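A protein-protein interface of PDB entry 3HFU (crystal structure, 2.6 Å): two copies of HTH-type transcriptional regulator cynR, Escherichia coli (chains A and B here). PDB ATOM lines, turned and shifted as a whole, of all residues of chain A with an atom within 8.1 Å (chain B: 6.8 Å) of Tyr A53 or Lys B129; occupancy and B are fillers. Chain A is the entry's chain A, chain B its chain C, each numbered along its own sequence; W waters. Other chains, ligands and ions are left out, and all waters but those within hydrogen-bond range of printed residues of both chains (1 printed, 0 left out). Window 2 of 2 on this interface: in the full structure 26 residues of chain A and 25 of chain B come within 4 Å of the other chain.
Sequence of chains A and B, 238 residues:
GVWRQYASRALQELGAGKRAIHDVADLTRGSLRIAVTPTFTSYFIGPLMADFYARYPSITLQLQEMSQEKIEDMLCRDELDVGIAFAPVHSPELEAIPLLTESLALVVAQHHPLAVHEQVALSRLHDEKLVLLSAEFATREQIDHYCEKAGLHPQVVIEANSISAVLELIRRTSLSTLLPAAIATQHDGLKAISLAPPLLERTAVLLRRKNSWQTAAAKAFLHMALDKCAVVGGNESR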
ATOM      1  N   GLY A  46      16.481 -11.870 -23.235  1.00  0.00           N
ATOM      2  CA  GLY A  46      16.674 -12.243 -24.625  1.00  0.00           C
ATOM      3  C   GLY A  46      17.319 -11.160 -25.467  1.00  0.00           C
ATOM      4  O   GLY A  46      18.408 -11.351 -26.016  1.00  0.00           O
ATOM      5  N   PRO A  47      16.655 -10.011 -25.611  1.00  0.00           N
ATOM      6  CA  PRO A  47      17.187  -8.897 -26.398  1.00  0.00           C
ATOM      7  C   PRO A  47      18.550  -8.419 -25.891  1.00  0.00           C
ATOM      8  O   PRO A  47      19.385  -7.969 -26.664  1.00  0.00           O
ATOM      9  CB  PRO A  47      16.116  -7.817 -26.233  1.00  0.00           C
ATOM     10  CG  PRO A  47      14.875  -8.600 -26.058  1.00  0.00           C
ATOM     11  CD  PRO A  47      15.295  -9.709 -25.134  1.00  0.00           C
ATOM     12  N   LEU A  48      18.758  -8.519 -24.585  1.00  0.00           N
ATOM     13  CA  LEU A  48      19.998  -8.084 -23.971  1.00  0.00           C
ATOM     14  C   LEU A  48      21.173  -9.002 -24.322  1.00  0.00           C
ATOM     15  O   LEU A  48      22.208  -8.541 -24.806  1.00  0.00           O
ATOM     16  CB  LEU A  48      19.805  -8.003 -22.454  1.00  0.00           C
ATOM     17  CG  LEU A  48      20.998  -7.659 -21.563  1.00  0.00           C
ATOM     18  CD1 LEU A  48      21.532  -6.278 -21.918  1.00  0.00           C
ATOM     19  CD2 LEU A  48      20.570  -7.713 -20.098  1.00  0.00           C
ATOM     20  N   MET A  49      21.027 -10.298 -24.078  1.00  0.00           N
ATOM     21  CA  MET A  49      22.102 -11.237 -24.391  1.00  0.00           C
ATOM     22  C   MET A  49      22.402 -11.239 -25.897  1.00  0.00           C
ATOM     23  O   MET A  49      23.539 -11.444 -26.313  1.00  0.00           O
ATOM     24  CB  MET A  49      21.732 -12.646 -23.928  1.00  0.00           C
ATOM     25  CG  MET A  49      21.651 -12.817 -22.416  1.00  0.00           C
ATOM     26  SD  MET A  49      21.262 -14.651 -21.932  1.00  0.00           S
ATOM     27  CE  MET A  49      22.812 -15.452 -22.733  1.00  0.00           C
ATOM     28  N   ALA A  50      21.376 -11.007 -26.709  1.00  0.00           N
ATOM     29  CA  ALA A  50      21.545 -10.966 -28.155  1.00  0.00           C
ATOM     30  C   ALA A  50      22.493  -9.835 -28.520  1.00  0.00           C
ATOM     31  O   ALA A  50      23.415 -10.010 -29.323  1.00  0.00           O
ATOM     32  CB  ALA A  50      20.211 -10.745 -28.823  1.00  0.00           C
ATOM     33  N   ASP A  51      22.253  -8.672 -27.923  1.00  0.00           N
ATOM     34  CA  ASP A  51      23.077  -7.499 -28.152  1.00  0.00           C
ATOM     35  C   ASP A  51      24.473  -7.693 -27.592  1.00  0.00           C
ATOM     36  O   ASP A  51      25.460  -7.332 -28.237  1.00  0.00           O
ATOM     37  CB  ASP A  51      22.439  -6.263 -27.521  1.00  0.00           C
ATOM     38  CG  ASP A  51      21.196  -5.811 -28.265  1.00  0.00           C
ATOM     39  OD1 ASP A  51      21.189  -5.895 -29.513  1.00  0.00           O
ATOM     40  OD2 ASP A  51      20.231  -5.362 -27.615  1.00  0.00           O
ATOM     41  N   PHE A  52      24.555  -8.258 -26.393  1.00  0.00           N
ATOM     42  CA  PHE A  52      25.847  -8.485 -25.762  1.00  0.00           C
ATOM     43  C   PHE A  52      26.695  -9.418 -26.600  1.00  0.00           C
ATOM     44  O   PHE A  52      27.881  -9.173 -26.793  1.00  0.00           O
ATOM     45  CB  PHE A  52      25.685  -9.093 -24.371  1.00  0.00           C
ATOM     46  CG  PHE A  52      26.964  -9.157 -23.593  1.00  0.00           C
ATOM     47  CD1 PHE A  52      27.496  -8.015 -23.017  1.00  0.00           C
ATOM     48  CD2 PHE A  52      27.643 -10.352 -23.450  1.00  0.00           C
ATOM     49  CE1 PHE A  52      28.688  -8.068 -22.308  1.00  0.00           C
ATOM     50  CE2 PHE A  52      28.836 -10.412 -22.743  1.00  0.00           C
ATOM     51  CZ  PHE A  52      29.358  -9.269 -22.172  1.00  0.00           C
ATOM     52  N   TYR A  53      26.090 -10.494 -27.093  1.00  0.00           N
ATOM     53  CA  TYR A  53      26.818 -11.448 -27.916  1.00  0.00           C
ATOM     54  C   TYR A  53      27.340 -10.795 -29.188  1.00  0.00           C
ATOM     55  O   TYR A  53      28.495 -10.983 -29.559  1.00  0.00           O
ATOM     56  CB  TYR A  53      25.939 -12.626 -28.324  1.00  0.00           C
ATOM     57  CG  TYR A  53      26.702 -13.576 -29.225  1.00  0.00           C
ATOM     58  CD1 TYR A  53      27.793 -14.301 -28.737  1.00  0.00           C
ATOM     59  CD2 TYR A  53      26.406 -13.678 -30.577  1.00  0.00           C
ATOM     60  CE1 TYR A  53      28.564 -15.086 -29.573  1.00  0.00           C
ATOM     61  CE2 TYR A  53      27.186 -14.472 -31.425  1.00  0.00           C
ATOM     62  CZ  TYR A  53      28.260 -15.166 -30.916  1.00  0.00           C
ATOM     63  OH  TYR A  53      29.056 -15.917 -31.753  1.00  0.00           O
ATOM     64  N   ALA A  54      26.477 -10.045 -29.864  1.00  0.00           N
ATOM     65  CA  ALA A  54      26.854  -9.380 -31.100  1.00  0.00           C
ATOM     66  C   ALA A  54      27.996  -8.404 -30.865  1.00  0.00           C
ATOM     67  O   ALA A  54      28.787  -8.149 -31.772  1.00  0.00           O
ATOM     68  CB  ALA A  54      25.654  -8.651 -31.690  1.00  0.00           C
ATOM     69  N   ARG A  55      28.087  -7.862 -29.653  1.00  0.00           N
ATOM     70  CA  ARG A  55      29.145  -6.913 -29.326  1.00  0.00           C
ATOM     71  C   ARG A  55      30.448  -7.590 -28.870  1.00  0.00           C
ATOM     72  O   ARG A  55      31.542  -7.147 -29.209  1.00  0.00           O
ATOM     73  CB  ARG A  55      28.664  -5.940 -28.247  1.00  0.00           C
ATOM     74  CG  ARG A  55      29.608  -4.775 -28.029  1.00  0.00           C
ATOM     75  CD  ARG A  55      28.954  -3.680 -27.211  1.00  0.00           C
ATOM     76  NE  ARG A  55      29.839  -2.531 -27.044  1.00  0.00           N
ATOM     77  CZ  ARG A  55      29.520  -1.433 -26.366  1.00  0.00           C
ATOM     78  NH1 ARG A  55      28.330  -1.329 -25.785  1.00  0.00           N
ATOM     79  NH2 ARG A  55      30.393  -0.439 -26.262  1.00  0.00           N
ATOM     80  N   TYR A  56      30.336  -8.667 -28.103  1.00  0.00           N
ATOM     81  CA  TYR A  56      31.516  -9.374 -27.621  1.00  0.00           C
ATOM     82  C   TYR A  56      31.337 -10.866 -27.896  1.00  0.00           C
ATOM     83  O   TYR A  56      31.241 -11.660 -26.965  1.00  0.00           O
ATOM     84  CB  TYR A  56      31.678  -9.163 -26.115  1.00  0.00           C
ATOM     85  CG  TYR A  56      31.542  -7.727 -25.638  1.00  0.00           C
ATOM     86  CD1 TYR A  56      32.558  -6.794 -25.846  1.00  0.00           C
ATOM     87  CD2 TYR A  56      30.387  -7.302 -24.977  1.00  0.00           C
ATOM     88  CE1 TYR A  56      32.425  -5.465 -25.403  1.00  0.00           C
ATOM     89  CE2 TYR A  56      30.241  -5.983 -24.532  1.00  0.00           C
ATOM     90  CZ  TYR A  56      31.261  -5.069 -24.746  1.00  0.00           C
ATOM     91  OH  TYR A  56      31.112  -3.767 -24.307  1.00  0.00           O
ATOM     92  N   PRO A  57      31.304 -11.261 -29.183  1.00  0.00           N
ATOM     93  CA  PRO A  57      31.131 -12.654 -29.630  1.00  0.00           C
ATOM     94  C   PRO A  57      32.097 -13.658 -28.994  1.00  0.00           C
ATOM     95  O   PRO A  57      31.826 -14.856 -28.940  1.00  0.00           O
ATOM     96  CB  PRO A  57      31.333 -12.556 -31.144  1.00  0.00           C
ATOM     97  CG  PRO A  57      30.913 -11.143 -31.463  1.00  0.00           C
ATOM     98  CD  PRO A  57      31.531 -10.367 -30.333  1.00  0.00           C
ATOM     99  N   SER A  58      33.218 -13.150 -28.510  1.00  0.00           N
ATOM    100  CA  SER A  58      34.257 -13.983 -27.908  1.00  0.00           C
ATOM    101  C   SER A  58      33.896 -14.502 -26.525  1.00  0.00           C
ATOM    102  O   SER A  58      34.531 -15.422 -26.002  1.00  0.00           O
ATOM    103  CB  SER A  58      35.579 -13.204 -27.816  1.00  0.00           C
ATOM    104  OG  SER A  58      36.084 -12.868 -29.095  1.00  0.00           O
ATOM    105  N   ILE A  59      32.893 -13.893 -25.917  1.00  0.00           N
ATOM    106  CA  ILE A  59      32.463 -14.322 -24.597  1.00  0.00           C
ATOM    107  C   ILE A  59      31.332 -15.343 -24.692  1.00  0.00           C
ATOM    108  O   ILE A  59      30.275 -15.062 -25.259  1.00  0.00           O
ATOM    109  CB  ILE A  59      31.981 -13.121 -23.778  1.00  0.00           C
ATOM    110  CG1 ILE A  59      33.125 -12.120 -23.626  1.00  0.00           C
ATOM    111  CG2 ILE A  59      31.457 -13.582 -22.424  1.00  0.00           C
ATOM    112  CD1 ILE A  59      32.685 -10.776 -23.091  1.00  0.00           C
ATOM    113  N   THR A  60      31.568 -16.533 -24.148  1.00  0.00           N
ATOM    114  CA  THR A  60      30.547 -17.577 -24.165  1.00  0.00           C
ATOM    115  C   THR A  60      29.600 -17.319 -22.999  1.00  0.00           C
ATOM    116  O   THR A  60      30.029 -17.025 -21.883  1.00  0.00           O
ATOM    117  CB  THR A  60      31.180 -18.985 -24.071  1.00  0.00           C
ATOM    118  OG1 THR A  60      32.089 -19.038 -22.968  1.00  0.00           O
ATOM    119  CG2 THR A  60      31.935 -19.291 -25.331  1.00  0.00           C
ATOM    120  N   LEU A  61      28.307 -17.433 -23.275  1.00  0.00           N
ATOM    121  CA  LEU A  61      27.281 -17.168 -22.278  1.00  0.00           C
ATOM    122  C   LEU A  61      26.489 -18.360 -21.753  1.00  0.00           C
ATOM    123  O   LEU A  61      26.148 -19.295 -22.489  1.00  0.00           O
ATOM    124  CB  LEU A  61      26.306 -16.138 -22.837  1.00  0.00           C
ATOM    125  CG  LEU A  61      27.008 -14.908 -23.416  1.00  0.00           C
ATOM    126  CD1 LEU A  61      25.965 -13.940 -23.998  1.00  0.00           C
ATOM    127  CD2 LEU A  61      27.851 -14.242 -22.327  1.00  0.00           C
ATOM    128  N   PHE A 221      28.289  -6.139 -19.109  1.00  0.00           N
ATOM    129  CA  PHE A 221      26.928  -6.662 -19.057  1.00  0.00           C
ATOM    130  C   PHE A 221      26.065  -5.691 -18.264  1.00  0.00           C
ATOM    131  O   PHE A 221      25.039  -5.196 -18.746  1.00  0.00           O
ATOM    132  CB  PHE A 221      26.888  -8.039 -18.386  1.00  0.00           C
ATOM    133  CG  PHE A 221      25.558  -8.717 -18.501  1.00  0.00           C
ATOM    134  CD1 PHE A 221      25.197  -9.371 -19.675  1.00  0.00           C
ATOM    135  CD2 PHE A 221      24.636  -8.646 -17.468  1.00  0.00           C
ATOM    136  CE1 PHE A 221      23.937  -9.940 -19.819  1.00  0.00           C
ATOM    137  CE2 PHE A 221      23.372  -9.212 -17.602  1.00  0.00           C
ATOM    138  CZ  PHE A 221      23.024  -9.859 -18.781  1.00  0.00           C
ATOM    139  N   MET A 224      25.369  -2.426 -20.101  1.00  0.00           N
ATOM    140  CA  MET A 224      24.355  -2.603 -21.136  1.00  0.00           C
ATOM    141  C   MET A 224      22.954  -2.796 -20.562  1.00  0.00           C
ATOM    142  O   MET A 224      22.000  -2.171 -21.029  1.00  0.00           O
ATOM    143  CB  MET A 224      24.713  -3.782 -22.050  1.00  0.00           C
ATOM    144  CG  MET A 224      25.895  -3.504 -22.980  1.00  0.00           C
ATOM    145  SD  MET A 224      26.163  -4.879 -24.324  1.00  0.00           S
ATOM    146  CE  MET A 224      24.288  -5.125 -24.744  1.00  0.00           C
ATOM    147  N   HIS B 112      19.537 -15.782 -41.560  1.00  0.00           N
ATOM    148  CA  HIS B 112      20.675 -16.655 -41.386  1.00  0.00           C
ATOM    149  C   HIS B 112      21.095 -17.107 -42.788  1.00  0.00           C
ATOM    150  O   HIS B 112      20.254 -17.469 -43.605  1.00  0.00           O
ATOM    151  CB  HIS B 112      20.272 -17.841 -40.511  1.00  0.00           C
ATOM    152  CG  HIS B 112      21.434 -18.591 -39.952  1.00  0.00           C
ATOM    153  ND1 HIS B 112      22.213 -19.433 -40.716  1.00  0.00           N
ATOM    154  CD2 HIS B 112      21.977 -18.589 -38.714  1.00  0.00           C
ATOM    155  CE1 HIS B 112      23.190 -19.917 -39.971  1.00  0.00           C
ATOM    156  NE2 HIS B 112      23.070 -19.420 -38.752  1.00  0.00           N
ATOM    157  N   LEU B 125      27.334 -28.536 -39.693  1.00  0.00           N
ATOM    158  CA  LEU B 125      27.361 -28.226 -38.274  1.00  0.00           C
ATOM    159  C   LEU B 125      28.726 -27.810 -37.756  1.00  0.00           C
ATOM    160  O   LEU B 125      28.823 -27.030 -36.805  1.00  0.00           O
ATOM    161  CB  LEU B 125      26.858 -29.422 -37.473  1.00  0.00           C
ATOM    162  CG  LEU B 125      25.383 -29.708 -37.706  1.00  0.00           C
ATOM    163  CD1 LEU B 125      24.919 -30.739 -36.695  1.00  0.00           C
ATOM    164  CD2 LEU B 125      24.589 -28.411 -37.577  1.00  0.00           C
ATOM    165  N   HIS B 126      29.785 -28.324 -38.371  1.00  0.00           N
ATOM    166  CA  HIS B 126      31.112 -27.963 -37.917  1.00  0.00           C
ATOM    167  C   HIS B 126      31.349 -26.456 -37.919  1.00  0.00           C
ATOM    168  O   HIS B 126      32.063 -25.937 -37.068  1.00  0.00           O
ATOM    169  CB  HIS B 126      32.187 -28.636 -38.765  1.00  0.00           C
ATOM    170  CG  HIS B 126      33.583 -28.302 -38.329  1.00  0.00           C
ATOM    171  ND1 HIS B 126      34.106 -27.029 -38.417  1.00  0.00           N
ATOM    172  CD2 HIS B 126      34.549 -29.064 -37.763  1.00  0.00           C
ATOM    173  CE1 HIS B 126      35.332 -27.021 -37.925  1.00  0.00           C
ATOM    174  NE2 HIS B 126      35.626 -28.244 -37.521  1.00  0.00           N
ATOM    175  N   ASP B 127      30.758 -25.737 -38.864  1.00  0.00           N
ATOM    176  CA  ASP B 127      30.991 -24.301 -38.921  1.00  0.00           C
ATOM    177  C   ASP B 127      29.943 -23.469 -38.225  1.00  0.00           C
ATOM    178  O   ASP B 127      30.047 -22.250 -38.186  1.00  0.00           O
ATOM    179  CB  ASP B 127      31.119 -23.844 -40.367  1.00  0.00           C
ATOM    180  CG  ASP B 127      32.303 -24.473 -41.068  1.00  0.00           C
ATOM    181  OD1 ASP B 127      33.410 -24.520 -40.484  1.00  0.00           O
ATOM    182  OD2 ASP B 127      32.133 -24.918 -42.221  1.00  0.00           O
ATOM    183  N   GLU B 128      28.932 -24.123 -37.670  1.00  0.00           N
ATOM    184  CA  GLU B 128      27.875 -23.405 -36.978  1.00  0.00           C
ATOM    185  C   GLU B 128      28.186 -23.100 -35.521  1.00  0.00           C
ATOM    186  O   GLU B 128      28.692 -23.948 -34.781  1.00  0.00           O
ATOM    187  CB  GLU B 128      26.561 -24.193 -37.033  1.00  0.00           C
ATOM    188  CG  GLU B 128      25.909 -24.216 -38.394  1.00  0.00           C
ATOM    189  CD  GLU B 128      25.572 -22.836 -38.878  1.00  0.00           C
ATOM    190  OE1 GLU B 128      24.916 -22.095 -38.119  1.00  0.00           O
ATOM    191  OE2 GLU B 128      25.958 -22.497 -40.017  1.00  0.00           O
ATOM    192  N   LYS B 129      27.895 -21.864 -35.130  1.00  0.00           N
ATOM    193  CA  LYS B 129      28.042 -21.439 -33.748  1.00  0.00           C
ATOM    194  C   LYS B 129      26.628 -21.549 -33.186  1.00  0.00           C
ATOM    195  O   LYS B 129      25.706 -20.862 -33.627  1.00  0.00           O
ATOM    196  CB  LYS B 129      28.598 -20.023 -33.683  1.00  0.00           C
ATOM    197  CG  LYS B 129      30.047 -20.031 -34.089  1.00  0.00           C
ATOM    198  CD  LYS B 129      30.743 -18.751 -33.767  1.00  0.00           C
ATOM    199  CE  LYS B 129      32.230 -18.906 -33.978  1.00  0.00           C
ATOM    200  NZ  LYS B 129      32.916 -17.625 -33.679  1.00  0.00           N
ATOM    201  N   LEU B 130      26.479 -22.455 -32.229  1.00  0.00           N
ATOM    202  CA  LEU B 130      25.196 -22.760 -31.636  1.00  0.00           C
ATOM    203  C   LEU B 130      24.833 -22.171 -30.287  1.00  0.00           C
ATOM    204  O   LEU B 130      25.680 -21.760 -29.487  1.00  0.00           O
ATOM    205  CB  LEU B 130      25.054 -24.277 -31.527  1.00  0.00           C
ATOM    206  CG  LEU B 130      25.410 -25.096 -32.764  1.00  0.00           C
ATOM    207  CD1 LEU B 130      25.763 -26.495 -32.308  1.00  0.00           C
ATOM    208  CD2 LEU B 130      24.244 -25.093 -33.777  1.00  0.00           C
ATOM    209  N   VAL B 131      23.527 -22.160 -30.060  1.00  0.00           N
ATOM    210  CA  VAL B 131      22.940 -21.732 -28.814  1.00  0.00           C
ATOM    211  C   VAL B 131      22.117 -22.972 -28.486  1.00  0.00           C
ATOM    212  O   VAL B 131      21.149 -23.283 -29.181  1.00  0.00           O
ATOM    213  CB  VAL B 131      22.022 -20.502 -28.992  1.00  0.00           C
ATOM    214  CG1 VAL B 131      21.316 -20.194 -27.683  1.00  0.00           C
ATOM    215  CG2 VAL B 131      22.847 -19.294 -29.411  1.00  0.00           C
ATOM    216  N   PRO B 154      30.370 -29.284 -33.039  1.00  0.00           N
ATOM    217  CA  PRO B 154      30.097 -27.861 -33.231  1.00  0.00           C
ATOM    218  C   PRO B 154      30.441 -27.082 -31.976  1.00  0.00           C
ATOM    219  O   PRO B 154      30.523 -27.651 -30.884  1.00  0.00           O
ATOM    220  CB  PRO B 154      28.599 -27.825 -33.536  1.00  0.00           C
ATOM    221  CG  PRO B 154      28.299 -29.213 -34.041  1.00  0.00           C
ATOM    222  CD  PRO B 154      29.143 -30.084 -33.163  1.00  0.00           C
ATOM    223  N   GLN B 155      30.644 -25.780 -32.139  1.00  0.00           N
ATOM    224  CA  GLN B 155      30.973 -24.915 -31.015  1.00  0.00           C
ATOM    225  C   GLN B 155      29.703 -24.322 -30.403  1.00  0.00           C
ATOM    226  O   GLN B 155      28.874 -23.744 -31.105  1.00  0.00           O
ATOM    227  CB  GLN B 155      31.896 -23.784 -31.469  1.00  0.00           C
ATOM    228  CG  GLN B 155      32.471 -23.005 -30.311  1.00  0.00           C
ATOM    229  CD  GLN B 155      33.205 -21.759 -30.736  1.00  0.00           C
ATOM    230  OE1 GLN B 155      33.798 -21.074 -29.906  1.00  0.00           O
ATOM    231  NE2 GLN B 155      33.168 -21.450 -32.030  1.00  0.00           N
ATOM    232  N   VAL B 156      29.553 -24.485 -29.093  1.00  0.00           N
ATOM    233  CA  VAL B 156      28.394 -23.951 -28.389  1.00  0.00           C
ATOM    234  C   VAL B 156      28.828 -22.635 -27.724  1.00  0.00           C
ATOM    235  O   VAL B 156      29.512 -22.629 -26.700  1.00  0.00           O
ATOM    236  CB  VAL B 156      27.858 -24.958 -27.318  1.00  0.00           C
ATOM    237  CG1 VAL B 156      26.601 -24.400 -26.655  1.00  0.00           C
ATOM    238  CG2 VAL B 156      27.538 -26.284 -27.971  1.00  0.00           C
ATOM    239  N   VAL B 157      28.436 -21.520 -28.334  1.00  0.00           N
ATOM    240  CA  VAL B 157      28.794 -20.208 -27.821  1.00  0.00           C
ATOM    241  C   VAL B 157      27.824 -19.716 -26.742  1.00  0.00           C
ATOM    242  O   VAL B 157      28.183 -18.889 -25.908  1.00  0.00           O
ATOM    243  CB  VAL B 157      28.872 -19.171 -28.975  1.00  0.00           C
ATOM    244  CG1 VAL B 157      30.061 -19.470 -29.857  1.00  0.00           C
ATOM    245  CG2 VAL B 157      27.606 -19.209 -29.800  1.00  0.00           C
ATOM    246  N   ILE B 158      26.597 -20.224 -26.760  1.00  0.00           N
ATOM    247  CA  ILE B 158      25.597 -19.836 -25.770  1.00  0.00           C
ATOM    248  C   ILE B 158      24.688 -21.000 -25.365  1.00  0.00           C
ATOM    249  O   ILE B 158      24.168 -21.718 -26.217  1.00  0.00           O
ATOM    250  CB  ILE B 158      24.697 -18.700 -26.293  1.00  0.00           C
ATOM    251  CG1 ILE B 158      25.541 -17.449 -26.545  1.00  0.00           C
ATOM    252  CG2 ILE B 158      23.562 -18.421 -25.295  1.00  0.00           C
ATOM    253  CD1 ILE B 158      24.778 -16.292 -27.181  1.00  0.00           C
ATOM    254  N   LEU B 169      17.056 -15.845 -28.677  1.00  0.00           N
ATOM    255  CA  LEU B 169      18.438 -15.560 -29.049  1.00  0.00           C
ATOM    256  C   LEU B 169      18.707 -15.765 -30.533  1.00  0.00           C
ATOM    257  O   LEU B 169      19.438 -14.986 -31.158  1.00  0.00           O
ATOM    258  CB  LEU B 169      19.391 -16.427 -28.219  1.00  0.00           C
ATOM    259  CG  LEU B 169      19.758 -15.769 -26.894  1.00  0.00           C
ATOM    260  CD1 LEU B 169      20.527 -16.717 -26.010  1.00  0.00           C
ATOM    261  CD2 LEU B 169      20.564 -14.519 -27.203  1.00  0.00           C
ATOM    262  N   THR B 173      20.013 -13.026 -33.657  1.00  0.00           N
ATOM    263  CA  THR B 173      21.415 -13.248 -34.001  1.00  0.00           C
ATOM    264  C   THR B 173      21.499 -14.068 -35.274  1.00  0.00           C
ATOM    265  O   THR B 173      20.484 -14.388 -35.887  1.00  0.00           O
ATOM    266  CB  THR B 173      22.149 -14.023 -32.881  1.00  0.00           C
ATOM    267  OG1 THR B 173      21.508 -15.294 -32.673  1.00  0.00           O
ATOM    268  CG2 THR B 173      22.124 -13.231 -31.580  1.00  0.00           C
ATOM    269  N   SER B 174      22.718 -14.400 -35.671  1.00  0.00           N
ATOM    270  CA  SER B 174      22.917 -15.215 -36.854  1.00  0.00           C
ATOM    271  C   SER B 174      23.439 -16.568 -36.422  1.00  0.00           C
ATOM    272  O   SER B 174      24.129 -17.259 -37.166  1.00  0.00           O
ATOM    273  CB  SER B 174      23.888 -14.547 -37.818  1.00  0.00           C
ATOM    274  OG  SER B 174      23.163 -13.817 -38.792  1.00  0.00           O
ATOM    275  N   LEU B 175      23.100 -16.924 -35.190  1.00  0.00           N
ATOM    276  CA  LEU B 175      23.479 -18.198 -34.607  1.00  0.00           C
ATOM    277  C   LEU B 175      22.371 -19.203 -34.921  1.00  0.00           C
ATOM    278  O   LEU B 175      21.295 -18.825 -35.392  1.00  0.00           O
ATOM    279  CB  LEU B 175      23.656 -18.037 -33.089  1.00  0.00           C
ATOM    280  CG  LEU B 175      24.748 -17.019 -32.663  1.00  0.00           C
ATOM    281  CD1 LEU B 175      24.706 -16.788 -31.156  1.00  0.00           C
ATOM    282  CD2 LEU B 175      26.141 -17.521 -33.084  1.00  0.00           C
ATOM    283  N   SER B 176      22.632 -20.485 -34.692  1.00  0.00           N
ATOM    284  CA  SER B 176      21.610 -21.496 -34.940  1.00  0.00           C
ATOM    285  C   SER B 176      21.461 -22.376 -33.714  1.00  0.00           C
ATOM    286  O   SER B 176      22.127 -22.157 -32.695  1.00  0.00           O
ATOM    287  CB  SER B 176      21.938 -22.351 -36.178  1.00  0.00           C
ATOM    288  OG  SER B 176      23.178 -23.029 -36.055  1.00  0.00           O
ATOM    289  N   THR B 177      20.580 -23.368 -33.816  1.00  0.00           N
ATOM    290  CA  THR B 177      20.332 -24.274 -32.708  1.00  0.00           C
ATOM    291  C   THR B 177      19.789 -25.581 -33.234  1.00  0.00           C
ATOM    292  O   THR B 177      19.366 -25.669 -34.385  1.00  0.00           O
ATOM    293  CB  THR B 177      19.294 -23.687 -31.735  1.00  0.00           C
ATOM    294  OG1 THR B 177      19.453 -24.292 -30.452  1.00  0.00           O
ATOM    295  CG2 THR B 177      17.877 -23.946 -32.237  1.00  0.00           C
HETATM  296  O   HOH W   1      32.008 -16.298 -31.504  1.00  0.00           O
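Water W1 lies within hydrogen-bond range of the side-chain amino group of Lys B129 (2.7 Å), the backbone carbonyl oxygen of Pro A57 (2.9 Å) and the side-chain hydroxyl of Tyr A53 (3.0 Å).
The backbone NH (N) of Ser B176 is in hydrogen-bond range of the backbone carbonyl oxygen (O) of Lys B129, 3.3 Å away. The backbone NH of Val B157 lies within hydrogen-bond range of the backbone carbonyl oxygen of Leu B130, at 3.0 Å. The backbone NH (N) of Ile B158 lies within hydrogen-bond range of the backbone carbonyl oxygen (O) of Leu B130, at 3.3 Å. The backbone carbonyl oxygen (O) of Leu B169 lies within hydrogen-bond range of the side-chain hydroxyl (OG1) of Thr B173 (2.6 Å). The side-chain hydroxyl (OG1) of Thr B173 lies close to the backbone NH (N) of Leu B175 (3.4 Å).
Of the 19 printed residues of chain B, 5 touch a printed residue of chain A. Hydrophobic or aromatic side chains of chain B within 4 Å of the printed part of chain A: Ile B158, Leu B169 and Leu B175. Hydrophobic or aromatic side chains of chain A that line the printed part of chain B: Met A49 and Tyr A53. Among the printed residues, 9 pairs touch across the chains.
Of the printed residues of chain B, Met A49 touches Ile B158 and Leu B169. Of the printed residues of chain B, Leu A61 touches Val B157 and Ile B158. Glu B128 touches none of the printed residues of chain A. Of chain A, only Tyr A53 comes within 4 Å of Lys B129. Of the printed residues of chain A, Val B157 touches Thr A60 and Leu A61. Of the printed residues of chain A, Leu B169 touches Met A49 (3.9 Å) and Ala A50 (3.6 Å).
No position is printed for both chains. Of the 9 pairs that touch across the chains among the printed residues, none has its exchanged pair printed and touching as well.
Among the printed residues, pairs that only touch across the chains: Thr A60 with Val B157 (3.2 Å), Leu A61 with Ile B158 (3.4 Å), Tyr A53 with Leu B175 (3.4 Å), Ala A50 with Leu B169 (3.6 Å), Tyr A53 with Lys B129 (3.9 Å), Tyr A53 with Ile B158 (3.9 Å), Met A49 with Leu B169 (3.9 Å) and Met A49 with Ile B158 (3.99 Å).
N of Leu A61 lies within hydrogen-bond range of O of Val B157 (3.0 Å).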
